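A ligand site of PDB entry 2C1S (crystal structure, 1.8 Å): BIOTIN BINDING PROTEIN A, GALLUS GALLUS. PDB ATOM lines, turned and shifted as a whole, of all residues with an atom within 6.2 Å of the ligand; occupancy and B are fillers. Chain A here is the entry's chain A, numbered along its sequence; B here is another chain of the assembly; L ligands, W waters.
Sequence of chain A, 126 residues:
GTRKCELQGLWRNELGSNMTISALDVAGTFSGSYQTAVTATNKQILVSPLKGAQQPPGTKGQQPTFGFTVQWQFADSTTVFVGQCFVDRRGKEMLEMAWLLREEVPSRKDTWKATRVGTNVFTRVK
OD1 of Asn 120 lies within hydrogen-bond range of N1 of the ligand, at 2.8 Å.
OG1 of Thr 36 lies within hydrogen-bond range of N2 of the ligand (2.8 Å).
An oxygen (O1) of the ligand sits at hydrogen-bond distance from the side-chain hydroxyl of Thr 39 (2.6 Å).
The side-chain hydroxyl (OG1) of Thr 79 lies within hydrogen-bond range of an oxygen (O4) of the ligand (2.5 Å).
The side-chain hydroxyl (OG) of Ser 77 sits at hydrogen-bond distance from an oxygen (O2) of the ligand (2.7 Å).
The side-chain hydroxyl (OG) of Ser 17 is in hydrogen-bond range of an oxygen (O3) of the ligand (2.8 Å).
The side-chain hydroxyl (OH) of Tyr 34 is in hydrogen-bond range of an oxygen (O3) of the ligand (2.7 Å).
N of Ala 40 is in hydrogen-bond range of O1 of the ligand (2.8 Å).
An oxygen (O3) of the ligand sits at hydrogen-bond distance from the side-chain amide nitrogen (ND2) of Asn 13, at 3.0 Å.
The side-chain hydroxyl (OH) of Tyr 34 sits at hydrogen-bond distance from the side-chain amide nitrogen (ND2) of Asn 13.
OG1 of Thr 39 sits at hydrogen-bond distance from OG1 of Thr 41 (2.7 Å).
N of Ser 17 sits at hydrogen-bond distance from OD1 of Asn 13 (3.1 Å).
The side-chain amide oxygen (OD1) of Asn 13 is in hydrogen-bond range of the backbone NH (N) of Leu 15 (2.9 Å).
The side-chain hydroxyl (OG) of Ser 17 lies within hydrogen-bond range of the backbone NH (N) of Ala 37.
The backbone carbonyl oxygen (O) of Arg 116 is in hydrogen-bond range of the backbone NH (N) of Leu 101.
O of Val 38 is in hydrogen-bond range of OG1 of Thr 36.
The indole nitrogen of Trp 99 lies close to the side-chain amide oxygen of Asn 120 (3.2 Å).
Leu 15 touches the ligand (CD1 to N1, 3.6 Å).
O of Val 38 touches C5 of the ligand (3.5 Å).
N of Thr 41 touches O1 of the ligand (3.7 Å).
CE2 of Trp 72 touches C3 of the ligand, at 3.6 Å.
Phe 74 touches the ligand (CZ to C3, 3.8 Å).
CB of Ala 75 touches O2 of the ligand, at 3.97 Å.
Phe 81 touches the ligand (CZ to S1, 3.9 Å).
Trp 99 touches the ligand.
Leu 101 touches the ligand.
Trp 112 of chain B touches the ligand (CZ3 to C6, 3.4 Å).
19 residues have an atom within 4 Å of the ligand: Asn 13, Leu 15, Ser 17, Tyr 34, Thr 36, Val 38, Thr 39, Ala 40, Thr 41, Trp 72, Phe 74, Ala 75, Ser 77, Thr 79, Phe 81, Trp 99, Leu 101, Asn 120 and Trp 112 of chain B.
The nearest printed residue that does not touch the ligand is Ala 37 (5.1 Å).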
ATOM      1  N   ASN A  13     -20.880 -20.416 -17.824  1.00  0.00           N
ATOM      2  CA  ASN A  13     -22.147 -21.122 -17.753  1.00  0.00           C
ATOM      3  C   ASN A  13     -22.095 -22.188 -16.677  1.00  0.00           C
ATOM      4  O   ASN A  13     -21.056 -22.368 -16.006  1.00  0.00           O
ATOM      5  CB  ASN A  13     -22.578 -21.689 -19.137  1.00  0.00           C
ATOM      6  CG  ASN A  13     -21.725 -22.844 -19.641  1.00  0.00           C
ATOM      7  OD1 ASN A  13     -21.061 -23.547 -18.885  1.00  0.00           O
ATOM      8  ND2 ASN A  13     -21.787 -23.071 -20.982  1.00  0.00           N
ATOM      9  N   LEU A  15     -21.900 -25.370 -16.727  1.00  0.00           N
ATOM     10  CA  LEU A  15     -21.019 -26.503 -16.944  1.00  0.00           C
ATOM     11  C   LEU A  15     -19.576 -26.158 -16.568  1.00  0.00           C
ATOM     12  O   LEU A  15     -18.707 -27.027 -16.554  1.00  0.00           O
ATOM     13  CB  LEU A  15     -21.055 -26.945 -18.414  1.00  0.00           C
ATOM     14  CG  LEU A  15     -22.394 -27.413 -18.969  1.00  0.00           C
ATOM     15  CD1 LEU A  15     -22.234 -27.915 -20.421  1.00  0.00           C
ATOM     16  CD2 LEU A  15     -22.999 -28.486 -18.080  1.00  0.00           C
ATOM     17  N   SER A  17     -17.988 -23.786 -18.374  1.00  0.00           N
ATOM     18  CA  SER A  17     -17.413 -23.173 -19.558  1.00  0.00           C
ATOM     19  C   SER A  17     -17.312 -21.648 -19.447  1.00  0.00           C
ATOM     20  O   SER A  17     -18.200 -20.985 -18.887  1.00  0.00           O
ATOM     21  CB  SER A  17     -18.244 -23.547 -20.807  1.00  0.00           C
ATOM     22  OG  SER A  17     -18.262 -24.951 -20.926  1.00  0.00           O
ATOM     23  N   TYR A  34     -14.065 -19.242 -26.767  1.00  0.00           N
ATOM     24  CA  TYR A  34     -14.921 -20.143 -25.983  1.00  0.00           C
ATOM     25  C   TYR A  34     -14.057 -21.249 -25.437  1.00  0.00           C
ATOM     26  O   TYR A  34     -13.409 -21.987 -26.202  1.00  0.00           O
ATOM     27  CB  TYR A  34     -16.045 -20.741 -26.876  1.00  0.00           C
ATOM     28  CG  TYR A  34     -17.219 -21.263 -26.076  1.00  0.00           C
ATOM     29  CD1 TYR A  34     -18.375 -20.495 -25.952  1.00  0.00           C
ATOM     30  CD2 TYR A  34     -17.161 -22.490 -25.393  1.00  0.00           C
ATOM     31  CE1 TYR A  34     -19.466 -20.936 -25.183  1.00  0.00           C
ATOM     32  CE2 TYR A  34     -18.256 -22.976 -24.606  1.00  0.00           C
ATOM     33  CZ  TYR A  34     -19.414 -22.167 -24.521  1.00  0.00           C
ATOM     34  OH  TYR A  34     -20.534 -22.550 -23.782  1.00  0.00           O
ATOM     35  N   GLN A  35     -14.032 -21.355 -24.104  1.00  0.00           N
ATOM     36  CA  GLN A  35     -13.295 -22.383 -23.398  1.00  0.00           C
ATOM     37  C   GLN A  35     -14.278 -23.361 -22.726  1.00  0.00           C
ATOM     38  O   GLN A  35     -14.724 -23.153 -21.570  1.00  0.00           O
ATOM     39  CB  GLN A  35     -12.406 -21.754 -22.325  1.00  0.00           C
ATOM     40  CG  GLN A  35     -11.481 -22.756 -21.650  1.00  0.00           C
ATOM     41  CD  GLN A  35     -10.316 -23.197 -22.541  1.00  0.00           C
ATOM     42  OE1 GLN A  35      -9.723 -22.377 -23.252  1.00  0.00           O
ATOM     43  NE2 GLN A  35      -9.991 -24.479 -22.520  1.00  0.00           N
ATOM     44  N   THR A  36     -14.612 -24.426 -23.433  1.00  0.00           N
ATOM     45  CA  THR A  36     -15.589 -25.358 -22.895  1.00  0.00           C
ATOM     46  C   THR A  36     -14.989 -26.210 -21.783  1.00  0.00           C
ATOM     47  O   THR A  36     -13.807 -26.586 -21.854  1.00  0.00           O
ATOM     48  CB  THR A  36     -16.239 -26.233 -24.046  1.00  0.00           C
ATOM     49  OG1 THR A  36     -17.171 -27.141 -23.459  1.00  0.00           O
ATOM     50  CG2 THR A  36     -15.200 -27.051 -24.815  1.00  0.00           C
ATOM     51  N   ALA A  37     -15.770 -26.489 -20.728  1.00  0.00           N
ATOM     52  CA  ALA A  37     -15.328 -27.343 -19.627  1.00  0.00           C
ATOM     53  C   ALA A  37     -15.452 -28.815 -19.948  1.00  0.00           C
ATOM     54  O   ALA A  37     -14.823 -29.659 -19.286  1.00  0.00           O
ATOM     55  CB  ALA A  37     -16.112 -27.024 -18.362  1.00  0.00           C
ATOM     56  N   VAL A  38     -16.274 -29.123 -20.950  1.00  0.00           N
ATOM     57  CA  VAL A  38     -16.660 -30.481 -21.305  1.00  0.00           C
ATOM     58  C   VAL A  38     -16.531 -30.735 -22.817  1.00  0.00           C
ATOM     59  O   VAL A  38     -16.562 -29.809 -23.625  1.00  0.00           O
ATOM     60  CB  VAL A  38     -18.120 -30.783 -20.826  1.00  0.00           C
ATOM     61  CG1 VAL A  38     -18.242 -30.624 -19.315  1.00  0.00           C
ATOM     62  CG2 VAL A  38     -19.093 -29.844 -21.480  1.00  0.00           C
ATOM     63  N   THR A  39     -16.347 -31.983 -23.190  1.00  0.00           N
ATOM     64  CA  THR A  39     -16.318 -32.369 -24.595  1.00  0.00           C
ATOM     65  C   THR A  39     -16.854 -33.775 -24.738  1.00  0.00           C
ATOM     66  O   THR A  39     -16.672 -34.623 -23.835  1.00  0.00           O
ATOM     67  CB  THR A  39     -14.880 -32.248 -25.198  1.00  0.00           C
ATOM     68  OG1 THR A  39     -14.878 -32.688 -26.557  1.00  0.00           O
ATOM     69  CG2 THR A  39     -13.912 -33.105 -24.409  1.00  0.00           C
ATOM     70  N   ALA A  40     -17.512 -34.035 -25.862  1.00  0.00           N
ATOM     71  CA  ALA A  40     -17.943 -35.386 -26.233  1.00  0.00           C
ATOM     72  C   ALA A  40     -16.802 -36.223 -26.840  1.00  0.00           C
ATOM     73  O   ALA A  40     -16.981 -37.415 -27.110  1.00  0.00           O
ATOM     74  CB  ALA A  40     -19.125 -35.331 -27.179  1.00  0.00           C
ATOM     75  N   THR A  41     -15.669 -35.577 -27.091  1.00  0.00           N
ATOM     76  CA  THR A  41     -14.471 -36.229 -27.624  1.00  0.00           C
ATOM     77  C   THR A  41     -13.568 -36.702 -26.489  1.00  0.00           C
ATOM     78  O   THR A  41     -13.854 -36.420 -25.321  1.00  0.00           O
ATOM     79  CB  THR A  41     -13.630 -35.277 -28.513  1.00  0.00           C
ATOM     80  OG1 THR A  41     -13.027 -34.216 -27.739  1.00  0.00           O
ATOM     81  CG2 THR A  41     -14.472 -34.680 -29.603  1.00  0.00           C
ATOM     82  N   TRP A  72     -14.659 -25.328 -32.979  1.00  0.00           N
ATOM     83  CA  TRP A  72     -13.839 -26.043 -32.000  1.00  0.00           C
ATOM     84  C   TRP A  72     -12.496 -26.358 -32.604  1.00  0.00           C
ATOM     85  O   TRP A  72     -12.437 -26.866 -33.717  1.00  0.00           O
ATOM     86  CB  TRP A  72     -14.508 -27.330 -31.539  1.00  0.00           C
ATOM     87  CG  TRP A  72     -15.875 -27.061 -30.953  1.00  0.00           C
ATOM     88  CD1 TRP A  72     -17.070 -27.380 -31.518  1.00  0.00           C
ATOM     89  CD2 TRP A  72     -16.176 -26.356 -29.718  1.00  0.00           C
ATOM     90  NE1 TRP A  72     -18.099 -26.958 -30.705  1.00  0.00           N
ATOM     91  CE2 TRP A  72     -17.592 -26.319 -29.601  1.00  0.00           C
ATOM     92  CE3 TRP A  72     -15.399 -25.779 -28.700  1.00  0.00           C
ATOM     93  CZ2 TRP A  72     -18.247 -25.726 -28.510  1.00  0.00           C
ATOM     94  CZ3 TRP A  72     -16.049 -25.201 -27.603  1.00  0.00           C
ATOM     95  CH2 TRP A  72     -17.462 -25.182 -27.517  1.00  0.00           C
ATOM     96  N   PHE A  74     -10.269 -28.448 -31.399  1.00  0.00           N
ATOM     97  CA  PHE A  74      -9.800 -29.731 -30.967  1.00  0.00           C
ATOM     98  C   PHE A  74     -10.791 -30.825 -31.387  1.00  0.00           C
ATOM     99  O   PHE A  74     -10.666 -31.961 -30.960  1.00  0.00           O
ATOM    100  CB  PHE A  74      -9.660 -29.731 -29.457  1.00  0.00           C
ATOM    101  CG  PHE A  74     -10.946 -29.394 -28.751  1.00  0.00           C
ATOM    102  CD1 PHE A  74     -11.787 -30.403 -28.291  1.00  0.00           C
ATOM    103  CD2 PHE A  74     -11.317 -28.062 -28.575  1.00  0.00           C
ATOM    104  CE1 PHE A  74     -12.997 -30.092 -27.673  1.00  0.00           C
ATOM    105  CE2 PHE A  74     -12.504 -27.754 -27.949  1.00  0.00           C
ATOM    106  CZ  PHE A  74     -13.347 -28.768 -27.502  1.00  0.00           C
ATOM    107  N   ALA A  75     -11.788 -30.438 -32.182  1.00  0.00           N
ATOM    108  CA  ALA A  75     -12.821 -31.371 -32.649  1.00  0.00           C
ATOM    109  C   ALA A  75     -13.341 -31.000 -34.038  1.00  0.00           C
ATOM    110  O   ALA A  75     -13.216 -29.856 -34.471  1.00  0.00           O
ATOM    111  CB  ALA A  75     -13.980 -31.442 -31.635  1.00  0.00           C
ATOM    112  N   ASP A  76     -13.905 -31.989 -34.736  1.00  0.00           N
ATOM    113  CA  ASP A  76     -14.447 -31.780 -36.081  1.00  0.00           C
ATOM    114  C   ASP A  76     -15.878 -31.256 -36.099  1.00  0.00           C
ATOM    115  O   ASP A  76     -16.440 -30.985 -37.138  1.00  0.00           O
ATOM    116  CB  ASP A  76     -14.308 -33.063 -36.895  1.00  0.00           C
ATOM    117  CG  ASP A  76     -12.873 -33.518 -36.967  1.00  0.00           C
ATOM    118  OD1 ASP A  76     -12.002 -32.622 -36.994  1.00  0.00           O
ATOM    119  OD2 ASP A  76     -12.589 -34.742 -36.967  1.00  0.00           O
ATOM    120  N   SER A  77     -16.421 -31.055 -34.910  1.00  0.00           N
ATOM    121  CA  SER A  77     -17.811 -30.680 -34.763  1.00  0.00           C
ATOM    122  C   SER A  77     -17.904 -29.149 -34.748  1.00  0.00           C
ATOM    123  O   SER A  77     -16.884 -28.452 -34.652  1.00  0.00           O
ATOM    124  CB  SER A  77     -18.295 -31.238 -33.433  1.00  0.00           C
ATOM    125  OG  SER A  77     -17.481 -30.694 -32.412  1.00  0.00           O
ATOM    126  N   THR A  78     -19.133 -28.629 -34.802  1.00  0.00           N
ATOM    127  CA  THR A  78     -19.399 -27.197 -34.757  1.00  0.00           C
ATOM    128  C   THR A  78     -20.602 -27.062 -33.854  1.00  0.00           C
ATOM    129  O   THR A  78     -21.513 -27.876 -33.919  1.00  0.00           O
ATOM    130  CB  THR A  78     -19.714 -26.598 -36.146  1.00  0.00           C
ATOM    131  OG1 THR A  78     -18.507 -26.627 -36.940  1.00  0.00           O
ATOM    132  CG2 THR A  78     -20.124 -25.174 -36.035  1.00  0.00           C
ATOM    133  N   THR A  79     -20.588 -26.029 -33.019  1.00  0.00           N
ATOM    134  CA  THR A  79     -21.750 -25.702 -32.181  1.00  0.00           C
ATOM    135  C   THR A  79     -22.302 -24.346 -32.560  1.00  0.00           C
ATOM    136  O   THR A  79     -21.539 -23.413 -32.816  1.00  0.00           O
ATOM    137  CB  THR A  79     -21.410 -25.688 -30.675  1.00  0.00           C
ATOM    138  OG1 THR A  79     -20.959 -26.971 -30.281  1.00  0.00           O
ATOM    139  CG2 THR A  79     -22.620 -25.332 -29.807  1.00  0.00           C
ATOM    140  N   VAL A  80     -23.632 -24.233 -32.541  1.00  0.00           N
ATOM    141  CA  VAL A  80     -24.281 -22.929 -32.608  1.00  0.00           C
ATOM    142  C   VAL A  80     -25.073 -22.684 -31.328  1.00  0.00           C
ATOM    143  O   VAL A  80     -25.740 -23.598 -30.811  1.00  0.00           O
ATOM    144  CB  VAL A  80     -25.141 -22.713 -33.895  1.00  0.00           C
ATOM    145  CG1 VAL A  80     -24.227 -22.699 -35.182  1.00  0.00           C
ATOM    146  CG2 VAL A  80     -26.283 -23.777 -33.995  1.00  0.00           C
ATOM    147  N   PHE A  81     -24.966 -21.467 -30.811  1.00  0.00           N
ATOM    148  CA  PHE A  81     -25.715 -21.019 -29.631  1.00  0.00           C
ATOM    149  C   PHE A  81     -26.642 -19.889 -30.037  1.00  0.00           C
ATOM    150  O   PHE A  81     -26.274 -18.986 -30.803  1.00  0.00           O
ATOM    151  CB  PHE A  81     -24.759 -20.461 -28.573  1.00  0.00           C
ATOM    152  CG  PHE A  81     -23.913 -21.498 -27.885  1.00  0.00           C
ATOM    153  CD1 PHE A  81     -24.286 -21.979 -26.633  1.00  0.00           C
ATOM    154  CD2 PHE A  81     -22.718 -21.959 -28.450  1.00  0.00           C
ATOM    155  CE1 PHE A  81     -23.494 -22.920 -25.973  1.00  0.00           C
ATOM    156  CE2 PHE A  81     -21.944 -22.903 -27.803  1.00  0.00           C
ATOM    157  CZ  PHE A  81     -22.323 -23.391 -26.547  1.00  0.00           C
ATOM    158  N   TRP A  99     -28.535 -24.527 -27.736  1.00  0.00           N
ATOM    159  CA  TRP A  99     -27.437 -24.832 -28.624  1.00  0.00           C
ATOM    160  C   TRP A  99     -27.686 -26.112 -29.404  1.00  0.00           C
ATOM    161  O   TRP A  99     -28.488 -26.961 -28.988  1.00  0.00           O
ATOM    162  CB  TRP A  99     -26.097 -24.891 -27.833  1.00  0.00           C
ATOM    163  CG  TRP A  99     -26.097 -25.868 -26.673  1.00  0.00           C
ATOM    164  CD1 TRP A  99     -26.176 -25.545 -25.346  1.00  0.00           C
ATOM    165  CD2 TRP A  99     -25.929 -27.287 -26.731  1.00  0.00           C
ATOM    166  NE1 TRP A  99     -26.094 -26.686 -24.585  1.00  0.00           N
ATOM    167  CE2 TRP A  99     -25.956 -27.767 -25.404  1.00  0.00           C
ATOM    168  CE3 TRP A  99     -25.757 -28.210 -27.792  1.00  0.00           C
ATOM    169  CZ2 TRP A  99     -25.835 -29.124 -25.086  1.00  0.00           C
ATOM    170  CZ3 TRP A  99     -25.630 -29.569 -27.466  1.00  0.00           C
ATOM    171  CH2 TRP A  99     -25.665 -30.012 -26.138  1.00  0.00           C
ATOM    172  N   LEU A 100     -27.007 -26.204 -30.554  1.00  0.00           N
ATOM    173  CA  LEU A 100     -26.925 -27.435 -31.339  1.00  0.00           C
ATOM    174  C   LEU A 100     -25.462 -27.745 -31.602  1.00  0.00           C
ATOM    175  O   LEU A 100     -24.718 -26.853 -32.015  1.00  0.00           O
ATOM    176  CB  LEU A 100     -27.654 -27.283 -32.686  1.00  0.00           C
ATOM    177  CG  LEU A 100     -29.171 -27.060 -32.743  1.00  0.00           C
ATOM    178  CD1 LEU A 100     -29.650 -26.723 -34.183  1.00  0.00           C
ATOM    179  CD2 LEU A 100     -29.923 -28.279 -32.181  1.00  0.00           C
ATOM    180  N   LEU A 101     -25.093 -28.996 -31.367  1.00  0.00           N
ATOM    181  CA  LEU A 101     -23.715 -29.467 -31.589  1.00  0.00           C
ATOM    182  C   LEU A 101     -23.792 -30.467 -32.723  1.00  0.00           C
ATOM    183  O   LEU A 101     -24.478 -31.505 -32.598  1.00  0.00           O
ATOM    184  CB  LEU A 101     -23.149 -30.076 -30.336  1.00  0.00           C
ATOM    185  CG  LEU A 101     -21.833 -30.875 -30.421  1.00  0.00           C
ATOM    186  CD1 LEU A 101     -20.672 -30.027 -30.863  1.00  0.00           C
ATOM    187  CD2 LEU A 101     -21.512 -31.561 -29.082  1.00  0.00           C
ATOM    188  N   GLU A 103     -21.928 -32.992 -35.131  1.00  0.00           N
ATOM    189  CA  GLU A 103     -20.821 -33.878 -35.510  1.00  0.00           C
ATOM    190  C   GLU A 103     -20.580 -33.949 -37.027  1.00  0.00           C
ATOM    191  O   GLU A 103     -21.523 -33.977 -37.827  1.00  0.00           O
ATOM    192  CB  GLU A 103     -21.181 -35.302 -35.092  1.00  0.00           C
ATOM    193  CG  GLU A 103     -20.584 -35.747 -33.801  1.00  0.00           C
ATOM    194  CD  GLU A 103     -20.815 -37.218 -33.564  1.00  0.00           C
ATOM    195  OE1 GLU A 103     -20.707 -38.001 -34.547  1.00  0.00           O
ATOM    196  OE2 GLU A 103     -21.108 -37.587 -32.408  1.00  0.00           O
ATOM    197  N   ARG A 116     -26.782 -32.882 -31.647  1.00  0.00           N
ATOM    198  CA  ARG A 116     -27.241 -32.854 -30.257  1.00  0.00           C
ATOM    199  C   ARG A 116     -27.783 -31.462 -29.956  1.00  0.00           C
ATOM    200  O   ARG A 116     -27.390 -30.479 -30.595  1.00  0.00           O
ATOM    201  CB  ARG A 116     -26.119 -33.201 -29.280  1.00  0.00           C
ATOM    202  CG  ARG A 116     -25.632 -34.628 -29.335  1.00  0.00           C
ATOM    203  CD  ARG A 116     -24.554 -34.772 -28.231  1.00  0.00           C
ATOM    204  NE  ARG A 116     -23.754 -35.986 -28.317  1.00  0.00           N
ATOM    205  CZ  ARG A 116     -22.618 -36.100 -29.002  1.00  0.00           C
ATOM    206  NH1 ARG A 116     -22.126 -35.055 -29.651  1.00  0.00           N
ATOM    207  NH2 ARG A 116     -21.948 -37.244 -29.016  1.00  0.00           N
ATOM    208  N   THR A 119     -29.249 -26.728 -23.547  1.00  0.00           N
ATOM    209  CA  THR A 119     -29.428 -25.347 -23.098  1.00  0.00           C
ATOM    210  C   THR A 119     -28.301 -25.013 -22.114  1.00  0.00           C
ATOM    211  O   THR A 119     -27.760 -25.907 -21.486  1.00  0.00           O
ATOM    212  CB  THR A 119     -30.815 -25.143 -22.386  1.00  0.00           C
ATOM    213  OG1 THR A 119     -30.872 -26.007 -21.222  1.00  0.00           O
ATOM    214  CG2 THR A 119     -32.011 -25.424 -23.333  1.00  0.00           C
ATOM    215  N   ASN A 120     -27.978 -23.743 -22.009  1.00  0.00           N
ATOM    216  CA  ASN A 120     -26.975 -23.262 -21.052  1.00  0.00           C
ATOM    217  C   ASN A 120     -27.480 -21.965 -20.508  1.00  0.00           C
ATOM    218  O   ASN A 120     -28.255 -21.232 -21.176  1.00  0.00           O
ATOM    219  CB  ASN A 120     -25.605 -23.053 -21.724  1.00  0.00           C
ATOM    220  CG  ASN A 120     -24.848 -24.347 -21.974  1.00  0.00           C
ATOM    221  OD1 ASN A 120     -24.299 -24.528 -23.048  1.00  0.00           O
ATOM    222  ND2 ASN A 120     -24.797 -25.240 -20.997  1.00  0.00           N
ATOM    223  N   PHE A 122     -25.602 -18.485 -18.893  1.00  0.00           N
ATOM    224  CA  PHE A 122     -24.329 -17.812 -18.621  1.00  0.00           C
ATOM    225  C   PHE A 122     -24.552 -16.640 -17.657  1.00  0.00           C
ATOM    226  O   PHE A 122     -25.576 -15.954 -17.723  1.00  0.00           O
ATOM    227  CB  PHE A 122     -23.710 -17.255 -19.900  1.00  0.00           C
ATOM    228  CG  PHE A 122     -23.232 -18.316 -20.889  1.00  0.00           C
ATOM    229  CD1 PHE A 122     -21.871 -18.655 -20.957  1.00  0.00           C
ATOM    230  CD2 PHE A 122     -24.145 -18.947 -21.769  1.00  0.00           C
ATOM    231  CE1 PHE A 122     -21.424 -19.593 -21.871  1.00  0.00           C
ATOM    232  CE2 PHE A 122     -23.702 -19.869 -22.689  1.00  0.00           C
ATOM    233  CZ  PHE A 122     -22.346 -20.201 -22.751  1.00  0.00           C
ATOM    234  N   TRP B 112     -25.474 -33.130 -20.458  1.00  0.00           N
ATOM    235  CA  TRP B 112     -25.491 -32.121 -21.522  1.00  0.00           C
ATOM    236  C   TRP B 112     -25.391 -32.760 -22.922  1.00  0.00           C
ATOM    237  O   TRP B 112     -25.941 -32.194 -23.868  1.00  0.00           O
ATOM    238  CB  TRP B 112     -24.368 -31.085 -21.364  1.00  0.00           C
ATOM    239  CG  TRP B 112     -23.013 -31.702 -21.602  1.00  0.00           C
ATOM    240  CD1 TRP B 112     -22.227 -32.349 -20.671  1.00  0.00           C
ATOM    241  CD2 TRP B 112     -22.334 -31.775 -22.836  1.00  0.00           C
ATOM    242  NE1 TRP B 112     -21.073 -32.801 -21.267  1.00  0.00           N
ATOM    243  CE2 TRP B 112     -21.120 -32.470 -22.597  1.00  0.00           C
ATOM    244  CE3 TRP B 112     -22.621 -31.315 -24.125  1.00  0.00           C
ATOM    245  CZ2 TRP B 112     -20.192 -32.708 -23.622  1.00  0.00           C
ATOM    246  CZ3 TRP B 112     -21.713 -31.574 -25.141  1.00  0.00           C
ATOM    247  CH2 TRP B 112     -20.489 -32.237 -24.876  1.00  0.00           C
HETATM  248  C1  LIG L   1     -17.194 -31.529 -28.961  1.00  0.00           C
HETATM  249  O1  LIG L   1     -17.029 -32.193 -27.917  1.00  0.00           O
HETATM  250  O2  LIG L   1     -17.578 -32.012 -30.045  1.00  0.00           O
HETATM  251  C2  LIG L   1     -16.905 -30.012 -28.953  1.00  0.00           C
HETATM  252  C3  LIG L   1     -17.130 -29.271 -27.616  1.00  0.00           C
HETATM  253  C4  LIG L   1     -18.623 -29.120 -27.379  1.00  0.00           C
HETATM  254  C5  LIG L   1     -18.874 -28.589 -25.955  1.00  0.00           C
HETATM  255  C6  LIG L   1     -20.400 -28.469 -25.726  1.00  0.00           C
HETATM  256  S1  LIG L   1     -21.209 -27.175 -26.687  1.00  0.00           S
HETATM  257  C7  LIG L   1     -22.731 -27.267 -25.700  1.00  0.00           C
HETATM  258  C8  LIG L   1     -22.258 -27.496 -24.258  1.00  0.00           C
HETATM  259  N1  LIG L   1     -22.056 -26.187 -23.602  1.00  0.00           N
HETATM  260  C9  LIG L   1     -20.763 -26.024 -23.294  1.00  0.00           C
HETATM  261  O3  LIG L   1     -20.379 -25.005 -22.709  1.00  0.00           O
HETATM  262  N2  LIG L   1     -19.985 -27.057 -23.628  1.00  0.00           N
HETATM  263  C10 LIG L   1     -20.828 -28.126 -24.251  1.00  0.00           C
HETATM  264  O4  LIG L   1     -21.488 -27.802 -28.019  1.00  0.00           O
HETATM  265  O   HOH W   1     -18.124 -34.548 -30.694  1.00  0.00           O
